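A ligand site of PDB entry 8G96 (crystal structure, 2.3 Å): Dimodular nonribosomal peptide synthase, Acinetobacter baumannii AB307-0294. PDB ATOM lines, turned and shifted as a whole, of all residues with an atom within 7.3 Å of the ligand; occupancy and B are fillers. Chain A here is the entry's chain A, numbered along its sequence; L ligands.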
ATOM      1  N   PHE A 194      -4.449 -20.168  -4.415  1.00  0.00           N
ATOM      2  CA  PHE A 194      -4.870 -21.114  -5.430  1.00  0.00           C
ATOM      3  C   PHE A 194      -5.367 -20.403  -6.678  1.00  0.00           C
ATOM      4  O   PHE A 194      -4.991 -20.754  -7.798  1.00  0.00           O
ATOM      5  CB  PHE A 194      -5.974 -22.038  -4.920  1.00  0.00           C
ATOM      6  CG  PHE A 194      -6.750 -22.681  -6.033  1.00  0.00           C
ATOM      7  CD1 PHE A 194      -6.250 -23.785  -6.672  1.00  0.00           C
ATOM      8  CD2 PHE A 194      -7.928 -22.106  -6.497  1.00  0.00           C
ATOM      9  CE1 PHE A 194      -6.925 -24.366  -7.731  1.00  0.00           C
ATOM     10  CE2 PHE A 194      -8.603 -22.673  -7.551  1.00  0.00           C
ATOM     11  CZ  PHE A 194      -8.104 -23.806  -8.179  1.00  0.00           C
ATOM     12  N   GLU A 198      -3.384 -21.373 -10.106  1.00  0.00           N
ATOM     13  CA  GLU A 198      -3.955 -22.156 -11.195  1.00  0.00           C
ATOM     14  C   GLU A 198      -4.250 -21.293 -12.416  1.00  0.00           C
ATOM     15  O   GLU A 198      -4.065 -21.738 -13.553  1.00  0.00           O
ATOM     16  CB  GLU A 198      -5.233 -22.878 -10.759  1.00  0.00           C
ATOM     17  CG  GLU A 198      -5.874 -23.610 -11.930  1.00  0.00           C
ATOM     18  CD  GLU A 198      -6.965 -24.595 -11.542  1.00  0.00           C
ATOM     19  OE1 GLU A 198      -8.111 -24.407 -12.006  1.00  0.00           O
ATOM     20  OE2 GLU A 198      -6.688 -25.560 -10.792  1.00  0.00           O
ATOM     21  N   PHE A 218     -19.112 -28.198  -4.377  1.00  0.00           N
ATOM     22  CA  PHE A 218     -17.991 -28.895  -4.981  1.00  0.00           C
ATOM     23  C   PHE A 218     -16.834 -27.946  -5.269  1.00  0.00           C
ATOM     24  O   PHE A 218     -17.042 -26.779  -5.621  1.00  0.00           O
ATOM     25  CB  PHE A 218     -18.413 -29.591  -6.282  1.00  0.00           C
ATOM     26  CG  PHE A 218     -19.381 -30.718  -6.063  1.00  0.00           C
ATOM     27  CD1 PHE A 218     -20.732 -30.476  -5.918  1.00  0.00           C
ATOM     28  CD2 PHE A 218     -18.923 -32.029  -6.009  1.00  0.00           C
ATOM     29  CE1 PHE A 218     -21.628 -31.517  -5.716  1.00  0.00           C
ATOM     30  CE2 PHE A 218     -19.810 -33.079  -5.803  1.00  0.00           C
ATOM     31  CZ  PHE A 218     -21.161 -32.825  -5.652  1.00  0.00           C
ATOM     32  N   ASP A 219     -15.609 -28.462  -5.111  1.00  0.00           N
ATOM     33  CA  ASP A 219     -14.416 -27.685  -5.394  1.00  0.00           C
ATOM     34  C   ASP A 219     -14.461 -27.016  -6.765  1.00  0.00           C
ATOM     35  O   ASP A 219     -14.085 -25.847  -6.898  1.00  0.00           O
ATOM     36  CB  ASP A 219     -13.177 -28.573  -5.302  1.00  0.00           C
ATOM     37  CG  ASP A 219     -12.777 -28.868  -3.863  1.00  0.00           C
ATOM     38  OD1 ASP A 219     -12.996 -27.990  -3.001  1.00  0.00           O
ATOM     39  OD2 ASP A 219     -12.246 -29.966  -3.590  1.00  0.00           O
ATOM     40  N   MET A 220     -14.913 -27.738  -7.796  1.00  0.00           N
ATOM     41  CA  MET A 220     -14.792 -27.199  -9.150  1.00  0.00           C
ATOM     42  C   MET A 220     -15.669 -25.968  -9.361  1.00  0.00           C
ATOM     43  O   MET A 220     -15.340 -25.137 -10.218  1.00  0.00           O
ATOM     44  CB  MET A 220     -15.127 -28.262 -10.197  1.00  0.00           C
ATOM     45  CG  MET A 220     -14.155 -29.438 -10.195  1.00  0.00           C
ATOM     46  SD  MET A 220     -14.013 -30.294 -11.784  1.00  0.00           S
ATOM     47  CE  MET A 220     -13.368 -28.985 -12.823  1.00  0.00           C
ATOM     48  N   GLU A 223     -13.351 -23.068  -9.439  1.00  0.00           N
ATOM     49  CA  GLU A 223     -12.722 -22.818 -10.724  1.00  0.00           C
ATOM     50  C   GLU A 223     -13.712 -22.199 -11.703  1.00  0.00           C
ATOM     51  O   GLU A 223     -13.324 -21.371 -12.534  1.00  0.00           O
ATOM     52  CB  GLU A 223     -12.136 -24.109 -11.290  1.00  0.00           C
ATOM     53  CG  GLU A 223     -11.137 -24.796 -10.366  1.00  0.00           C
ATOM     54  CD  GLU A 223     -10.753 -26.188 -10.847  1.00  0.00           C
ATOM     55  OE1 GLU A 223      -9.656 -26.345 -11.433  1.00  0.00           O
ATOM     56  OE2 GLU A 223     -11.552 -27.122 -10.674  1.00  0.00           O
ATOM     57  N   HIS A 262     -15.437 -26.051 -17.286  1.00  0.00           N
ATOM     58  CA  HIS A 262     -14.952 -26.903 -16.210  1.00  0.00           C
ATOM     59  C   HIS A 262     -15.951 -28.046 -16.057  1.00  0.00           C
ATOM     60  O   HIS A 262     -17.161 -27.816 -15.971  1.00  0.00           O
ATOM     61  CB  HIS A 262     -14.834 -26.120 -14.903  1.00  0.00           C
ATOM     62  CG  HIS A 262     -13.987 -24.884 -15.003  1.00  0.00           C
ATOM     63  ND1 HIS A 262     -12.613 -24.921 -14.929  1.00  0.00           N
ATOM     64  CD2 HIS A 262     -14.317 -23.588 -15.194  1.00  0.00           C
ATOM     65  CE1 HIS A 262     -12.132 -23.699 -15.059  1.00  0.00           C
ATOM     66  NE2 HIS A 262     -13.145 -22.873 -15.214  1.00  0.00           N
ATOM     67  N   ALA A 263     -15.441 -29.275 -16.050  1.00  0.00           N
ATOM     68  CA  ALA A 263     -16.326 -30.430 -16.061  1.00  0.00           C
ATOM     69  C   ALA A 263     -15.567 -31.668 -15.625  1.00  0.00           C
ATOM     70  O   ALA A 263     -14.336 -31.651 -15.483  1.00  0.00           O
ATOM     71  CB  ALA A 263     -16.956 -30.644 -17.438  1.00  0.00           C
ATOM     72  N   VAL A 264     -16.308 -32.745 -15.408  1.00  0.00           N
ATOM     73  CA  VAL A 264     -15.735 -34.069 -15.168  1.00  0.00           C
ATOM     74  C   VAL A 264     -15.732 -34.839 -16.484  1.00  0.00           C
ATOM     75  O   VAL A 264     -16.566 -34.561 -17.354  1.00  0.00           O
ATOM     76  CB  VAL A 264     -16.496 -34.814 -14.060  1.00  0.00           C
ATOM     77  CG1 VAL A 264     -16.651 -33.930 -12.829  1.00  0.00           C
ATOM     78  CG2 VAL A 264     -17.855 -35.271 -14.572  1.00  0.00           C
ATOM     79  N   ASN A 282     -11.455 -27.722 -18.798  1.00  0.00           N
ATOM     80  CA  ASN A 282     -10.780 -28.115 -17.566  1.00  0.00           C
ATOM     81  C   ASN A 282     -11.519 -29.317 -16.996  1.00  0.00           C
ATOM     82  O   ASN A 282     -12.639 -29.184 -16.481  1.00  0.00           O
ATOM     83  CB  ASN A 282     -10.720 -26.953 -16.573  1.00  0.00           C
ATOM     84  CG  ASN A 282     -10.179 -27.368 -15.208  1.00  0.00           C
ATOM     85  OD1 ASN A 282      -9.355 -28.271 -15.109  1.00  0.00           O
ATOM     86  ND2 ASN A 282     -10.634 -26.686 -14.156  1.00  0.00           N
ATOM     87  N   LEU A 283     -10.909 -30.500 -17.091  1.00  0.00           N
ATOM     88  CA  LEU A 283     -11.487 -31.730 -16.594  1.00  0.00           C
ATOM     89  C   LEU A 283     -10.876 -32.083 -15.245  1.00  0.00           C
ATOM     90  O   LEU A 283      -9.653 -32.246 -15.135  1.00  0.00           O
ATOM     91  CB  LEU A 283     -11.289 -32.884 -17.582  1.00  0.00           C
ATOM     92  CG  LEU A 283     -11.938 -32.697 -18.958  1.00  0.00           C
ATOM     93  CD1 LEU A 283     -11.636 -33.878 -19.866  1.00  0.00           C
ATOM     94  CD2 LEU A 283     -13.444 -32.505 -18.810  1.00  0.00           C
ATOM     95  N   GLY A 284     -11.719 -32.190 -14.217  1.00  0.00           N
ATOM     96  CA  GLY A 284     -11.271 -32.593 -12.898  1.00  0.00           C
ATOM     97  C   GLY A 284     -12.130 -33.733 -12.366  1.00  0.00           C
ATOM     98  O   GLY A 284     -13.143 -34.104 -12.946  1.00  0.00           O
ATOM     99  N   GLY A 285     -11.697 -34.273 -11.227  1.00  0.00           N
ATOM    100  CA  GLY A 285     -12.454 -35.287 -10.523  1.00  0.00           C
ATOM    101  C   GLY A 285     -12.035 -36.712 -10.825  1.00  0.00           C
ATOM    102  O   GLY A 285     -11.924 -37.536  -9.906  1.00  0.00           O
ATOM    103  N   GLU A 286     -11.806 -37.027 -12.101  1.00  0.00           N
ATOM    104  CA  GLU A 286     -11.309 -38.332 -12.499  1.00  0.00           C
ATOM    105  C   GLU A 286     -10.267 -38.154 -13.578  1.00  0.00           C
ATOM    106  O   GLU A 286     -10.356 -37.229 -14.392  1.00  0.00           O
ATOM    107  CB  GLU A 286     -12.449 -39.245 -12.972  1.00  0.00           C
ATOM    108  CG  GLU A 286     -13.154 -38.778 -14.230  1.00  0.00           C
ATOM    109  CD  GLU A 286     -14.636 -39.118 -14.244  1.00  0.00           C
ATOM    110  OE1 GLU A 286     -15.368 -38.590 -15.116  1.00  0.00           O
ATOM    111  OE2 GLU A 286     -15.072 -39.893 -13.375  1.00  0.00           O
ATOM    112  N   ASN A 305      -6.418 -31.379 -17.377  1.00  0.00           N
ATOM    113  CA  ASN A 305      -6.821 -32.393 -16.406  1.00  0.00           C
ATOM    114  C   ASN A 305      -6.231 -31.984 -15.067  1.00  0.00           C
ATOM    115  O   ASN A 305      -5.009 -31.976 -14.904  1.00  0.00           O
ATOM    116  CB  ASN A 305      -6.344 -33.784 -16.836  1.00  0.00           C
ATOM    117  CG  ASN A 305      -7.037 -34.908 -16.075  1.00  0.00           C
ATOM    118  OD1 ASN A 305      -6.425 -35.915 -15.730  1.00  0.00           O
ATOM    119  ND2 ASN A 305      -8.317 -34.726 -15.796  1.00  0.00           N
ATOM    120  N   THR A 306      -7.085 -31.586 -14.131  1.00  0.00           N
ATOM    121  CA  THR A 306      -6.652 -31.121 -12.834  1.00  0.00           C
ATOM    122  C   THR A 306      -6.909 -32.188 -11.773  1.00  0.00           C
ATOM    123  O   THR A 306      -7.936 -32.865 -11.802  1.00  0.00           O
ATOM    124  CB  THR A 306      -7.360 -29.814 -12.427  1.00  0.00           C
ATOM    125  OG1 THR A 306      -8.766 -29.940 -12.677  1.00  0.00           O
ATOM    126  CG2 THR A 306      -6.824 -28.634 -13.229  1.00  0.00           C
ATOM    127  N   TYR A 307      -5.976 -32.308 -10.840  1.00  0.00           N
ATOM    128  CA  TYR A 307      -6.085 -33.269  -9.755  1.00  0.00           C
ATOM    129  C   TYR A 307      -5.760 -32.566  -8.455  1.00  0.00           C
ATOM    130  O   TYR A 307      -4.959 -31.627  -8.411  1.00  0.00           O
ATOM    131  CB  TYR A 307      -5.140 -34.483  -9.966  1.00  0.00           C
ATOM    132  CG  TYR A 307      -4.766 -35.247  -8.704  1.00  0.00           C
ATOM    133  CD1 TYR A 307      -3.714 -34.827  -7.887  1.00  0.00           C
ATOM    134  CD2 TYR A 307      -5.458 -36.394  -8.328  1.00  0.00           C
ATOM    135  CE1 TYR A 307      -3.371 -35.517  -6.742  1.00  0.00           C
ATOM    136  CE2 TYR A 307      -5.119 -37.096  -7.175  1.00  0.00           C
ATOM    137  CZ  TYR A 307      -4.075 -36.651  -6.379  1.00  0.00           C
ATOM    138  OH  TYR A 307      -3.732 -37.341  -5.233  1.00  0.00           O
ATOM    139  N   GLY A 308      -6.387 -33.020  -7.374  1.00  0.00           N
ATOM    140  CA  GLY A 308      -6.055 -32.533  -6.058  1.00  0.00           C
ATOM    141  C   GLY A 308      -7.179 -32.745  -5.059  1.00  0.00           C
ATOM    142  O   GLY A 308      -8.362 -32.627  -5.383  1.00  0.00           O
ATOM    143  N   PRO A 309      -6.807 -33.064  -3.827  1.00  0.00           N
ATOM    144  CA  PRO A 309      -7.807 -33.209  -2.768  1.00  0.00           C
ATOM    145  C   PRO A 309      -8.325 -31.870  -2.292  1.00  0.00           C
ATOM    146  O   PRO A 309      -7.653 -30.830  -2.391  1.00  0.00           O
ATOM    147  CB  PRO A 309      -7.035 -33.935  -1.656  1.00  0.00           C
ATOM    148  CG  PRO A 309      -5.612 -33.530  -1.879  1.00  0.00           C
ATOM    149  CD  PRO A 309      -5.454 -33.402  -3.369  1.00  0.00           C
ATOM    150  N   THR A 310      -9.546 -31.892  -1.758  1.00  0.00           N
ATOM    151  CA  THR A 310     -10.142 -30.705  -1.167  1.00  0.00           C
ATOM    152  C   THR A 310      -9.249 -30.081  -0.098  1.00  0.00           C
ATOM    153  O   THR A 310      -9.270 -28.855   0.086  1.00  0.00           O
ATOM    154  CB  THR A 310     -11.513 -31.064  -0.576  1.00  0.00           C
ATOM    155  OG1 THR A 310     -12.347 -31.612  -1.607  1.00  0.00           O
ATOM    156  CG2 THR A 310     -12.200 -29.817   0.002  1.00  0.00           C
ATOM    157  N   GLU A 311      -8.466 -30.891   0.611  1.00  0.00           N
ATOM    158  CA  GLU A 311      -7.591 -30.445   1.697  1.00  0.00           C
ATOM    159  C   GLU A 311      -6.442 -29.545   1.243  1.00  0.00           C
ATOM    160  O   GLU A 311      -5.695 -29.054   2.105  1.00  0.00           O
ATOM    161  CB  GLU A 311      -7.022 -31.652   2.444  1.00  0.00           C
ATOM    162  CG  GLU A 311      -7.993 -32.388   3.336  1.00  0.00           C
ATOM    163  CD  GLU A 311      -8.831 -33.403   2.589  1.00  0.00           C
ATOM    164  OE1 GLU A 311      -8.976 -33.267   1.354  1.00  0.00           O
ATOM    165  OE2 GLU A 311      -9.316 -34.345   3.241  1.00  0.00           O
ATOM    166  N   THR A 313      -7.035 -27.069  -1.320  1.00  0.00           N
ATOM    167  CA  THR A 313      -7.708 -26.013  -2.056  1.00  0.00           C
ATOM    168  C   THR A 313      -7.867 -26.334  -3.534  1.00  0.00           C
ATOM    169  O   THR A 313      -6.986 -26.034  -4.352  1.00  0.00           O
ATOM    170  CB  THR A 313      -6.959 -24.693  -1.862  1.00  0.00           C
ATOM    171  OG1 THR A 313      -6.551 -24.574  -0.482  1.00  0.00           O
ATOM    172  CG2 THR A 313      -7.864 -23.508  -2.233  1.00  0.00           C
ATOM    173  N   VAL A 314      -9.000 -26.960  -3.871  1.00  0.00           N
ATOM    174  CA  VAL A 314      -9.506 -27.087  -5.236  1.00  0.00           C
ATOM    175  C   VAL A 314      -8.659 -27.994  -6.122  1.00  0.00           C
ATOM    176  O   VAL A 314      -9.115 -29.072  -6.525  1.00  0.00           O
ATOM    177  CB  VAL A 314      -9.688 -25.706  -5.877  1.00  0.00           C
ATOM    178  CG1 VAL A 314     -10.323 -25.833  -7.260  1.00  0.00           C
ATOM    179  CG2 VAL A 314     -10.536 -24.826  -4.981  1.00  0.00           C
ATOM    180  N   SER A 315      -7.433 -27.569  -6.446  1.00  0.00           N
ATOM    181  CA  SER A 315      -6.526 -28.427  -7.215  1.00  0.00           C
ATOM    182  C   SER A 315      -5.110 -28.332  -6.653  1.00  0.00           C
ATOM    183  O   SER A 315      -4.758 -27.367  -5.961  1.00  0.00           O
ATOM    184  CB  SER A 315      -6.515 -28.051  -8.709  1.00  0.00           C
ATOM    185  OG  SER A 315      -7.829 -27.880  -9.208  1.00  0.00           O
ATOM    186  N   ALA A 316      -4.298 -29.337  -6.969  1.00  0.00           N
ATOM    187  CA  ALA A 316      -2.919 -29.398  -6.510  1.00  0.00           C
ATOM    188  C   ALA A 316      -1.964 -29.622  -7.661  1.00  0.00           C
ATOM    189  O   ALA A 316      -0.793 -29.220  -7.603  1.00  0.00           O
ATOM    190  CB  ALA A 316      -2.748 -30.503  -5.461  1.00  0.00           C
ATOM    191  N   SER A 317      -2.445 -30.256  -8.735  1.00  0.00           N
ATOM    192  CA  SER A 317      -1.644 -30.442  -9.924  1.00  0.00           C
ATOM    193  C   SER A 317      -2.531 -30.279 -11.147  1.00  0.00           C
ATOM    194  O   SER A 317      -3.754 -30.379 -11.067  1.00  0.00           O
ATOM    195  CB  SER A 317      -0.962 -31.812  -9.942  1.00  0.00           C
ATOM    196  OG  SER A 317      -1.892 -32.854 -10.140  1.00  0.00           O
HETATM  197  N1  LIG L   1     -10.648 -31.212  -5.967  1.00  0.00           N
HETATM  198  C1  LIG L   1     -11.401 -31.931  -6.995  1.00  0.00           C
HETATM  199  C2  LIG L   1     -10.458 -32.499  -8.067  1.00  0.00           C
HETATM  200  C3  LIG L   1      -9.631 -31.385  -8.680  1.00  0.00           C
HETATM  201  C4  LIG L   1     -10.487 -30.466  -9.568  1.00  0.00           C
HETATM  202  N2  LIG L   1      -9.873 -29.249 -10.014  1.00  0.00           N
HETATM  203  C5  LIG L   1     -12.277 -33.046  -6.345  1.00  0.00           C
HETATM  204  O1  LIG L   1     -12.154 -33.232  -5.103  1.00  0.00           O
HETATM  205  O2  LIG L   1     -13.093 -33.654  -7.101  1.00  0.00           O
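Met 220 touches the ligand (CG to C4, 3.9 Å). Gly 285 touches the ligand. Thr 310 touches the ligand. Nine residues have an atom within 4 Å of the ligand: Asp 219, Met 220, Glu 223, Gly 285, Thr 306, Gly 308, Thr 310, Val 314 and Ser 315. Along chain A the residues within 4 Å of the ligand span positions 219 to 315. The nearest printed residue that does not touch the ligand is Gly 284 (4.03 Å).
OE1 of Glu 223 lies within hydrogen-bond range of OG of Ser 315 (3.3 Å). The side-chain carboxylate (OE2) of Glu 198 sits at hydrogen-bond distance from the side-chain hydroxyl (OG) of Ser 315 (3.0 Å). OE1 of Glu 223 is in hydrogen-bond range of ND2 of Asn 282, at 2.9 Å. OE1 of Glu 198 lies close to OE1 of Glu 223 (2.5 Å). A ring nitrogen (NE2) of His 262 sits at hydrogen-bond distance from the backbone carbonyl oxygen of Glu 223. OG1 of Thr 306 sits at hydrogen-bond distance from OD1 of Asn 282, 3.0 Å away. The backbone NH (N) of Thr 306 sits at hydrogen-bond distance from the backbone carbonyl oxygen (O) of Leu 283, 2.8 Å away. The side-chain carboxylate of Asp 219 lies within hydrogen-bond range of the side-chain hydroxyl of Thr 310 (2.6 Å).
N2 of the ligand is in hydrogen-bond range of OG of Ser 315 (2.6 Å). The backbone carbonyl oxygen (O) of Val 314 is in hydrogen-bond range of a nitrogen (N1) of the ligand. The backbone carbonyl oxygen of Gly 308 sits at hydrogen-bond distance from a nitrogen (N1) of the ligand, 2.8 Å away. The side-chain carboxylate of Glu 223 lies within salt-bridge range of a nitrogen (N2) of the ligand (2.8 Å). N2 of the ligand lies within hydrogen-bond range of OG1 of Thr 306, at 3.0 Å. A nitrogen (N1) of the ligand lies within salt-bridge range of the side-chain carboxylate (OD2) of Asp 219, at 3.1 Å.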
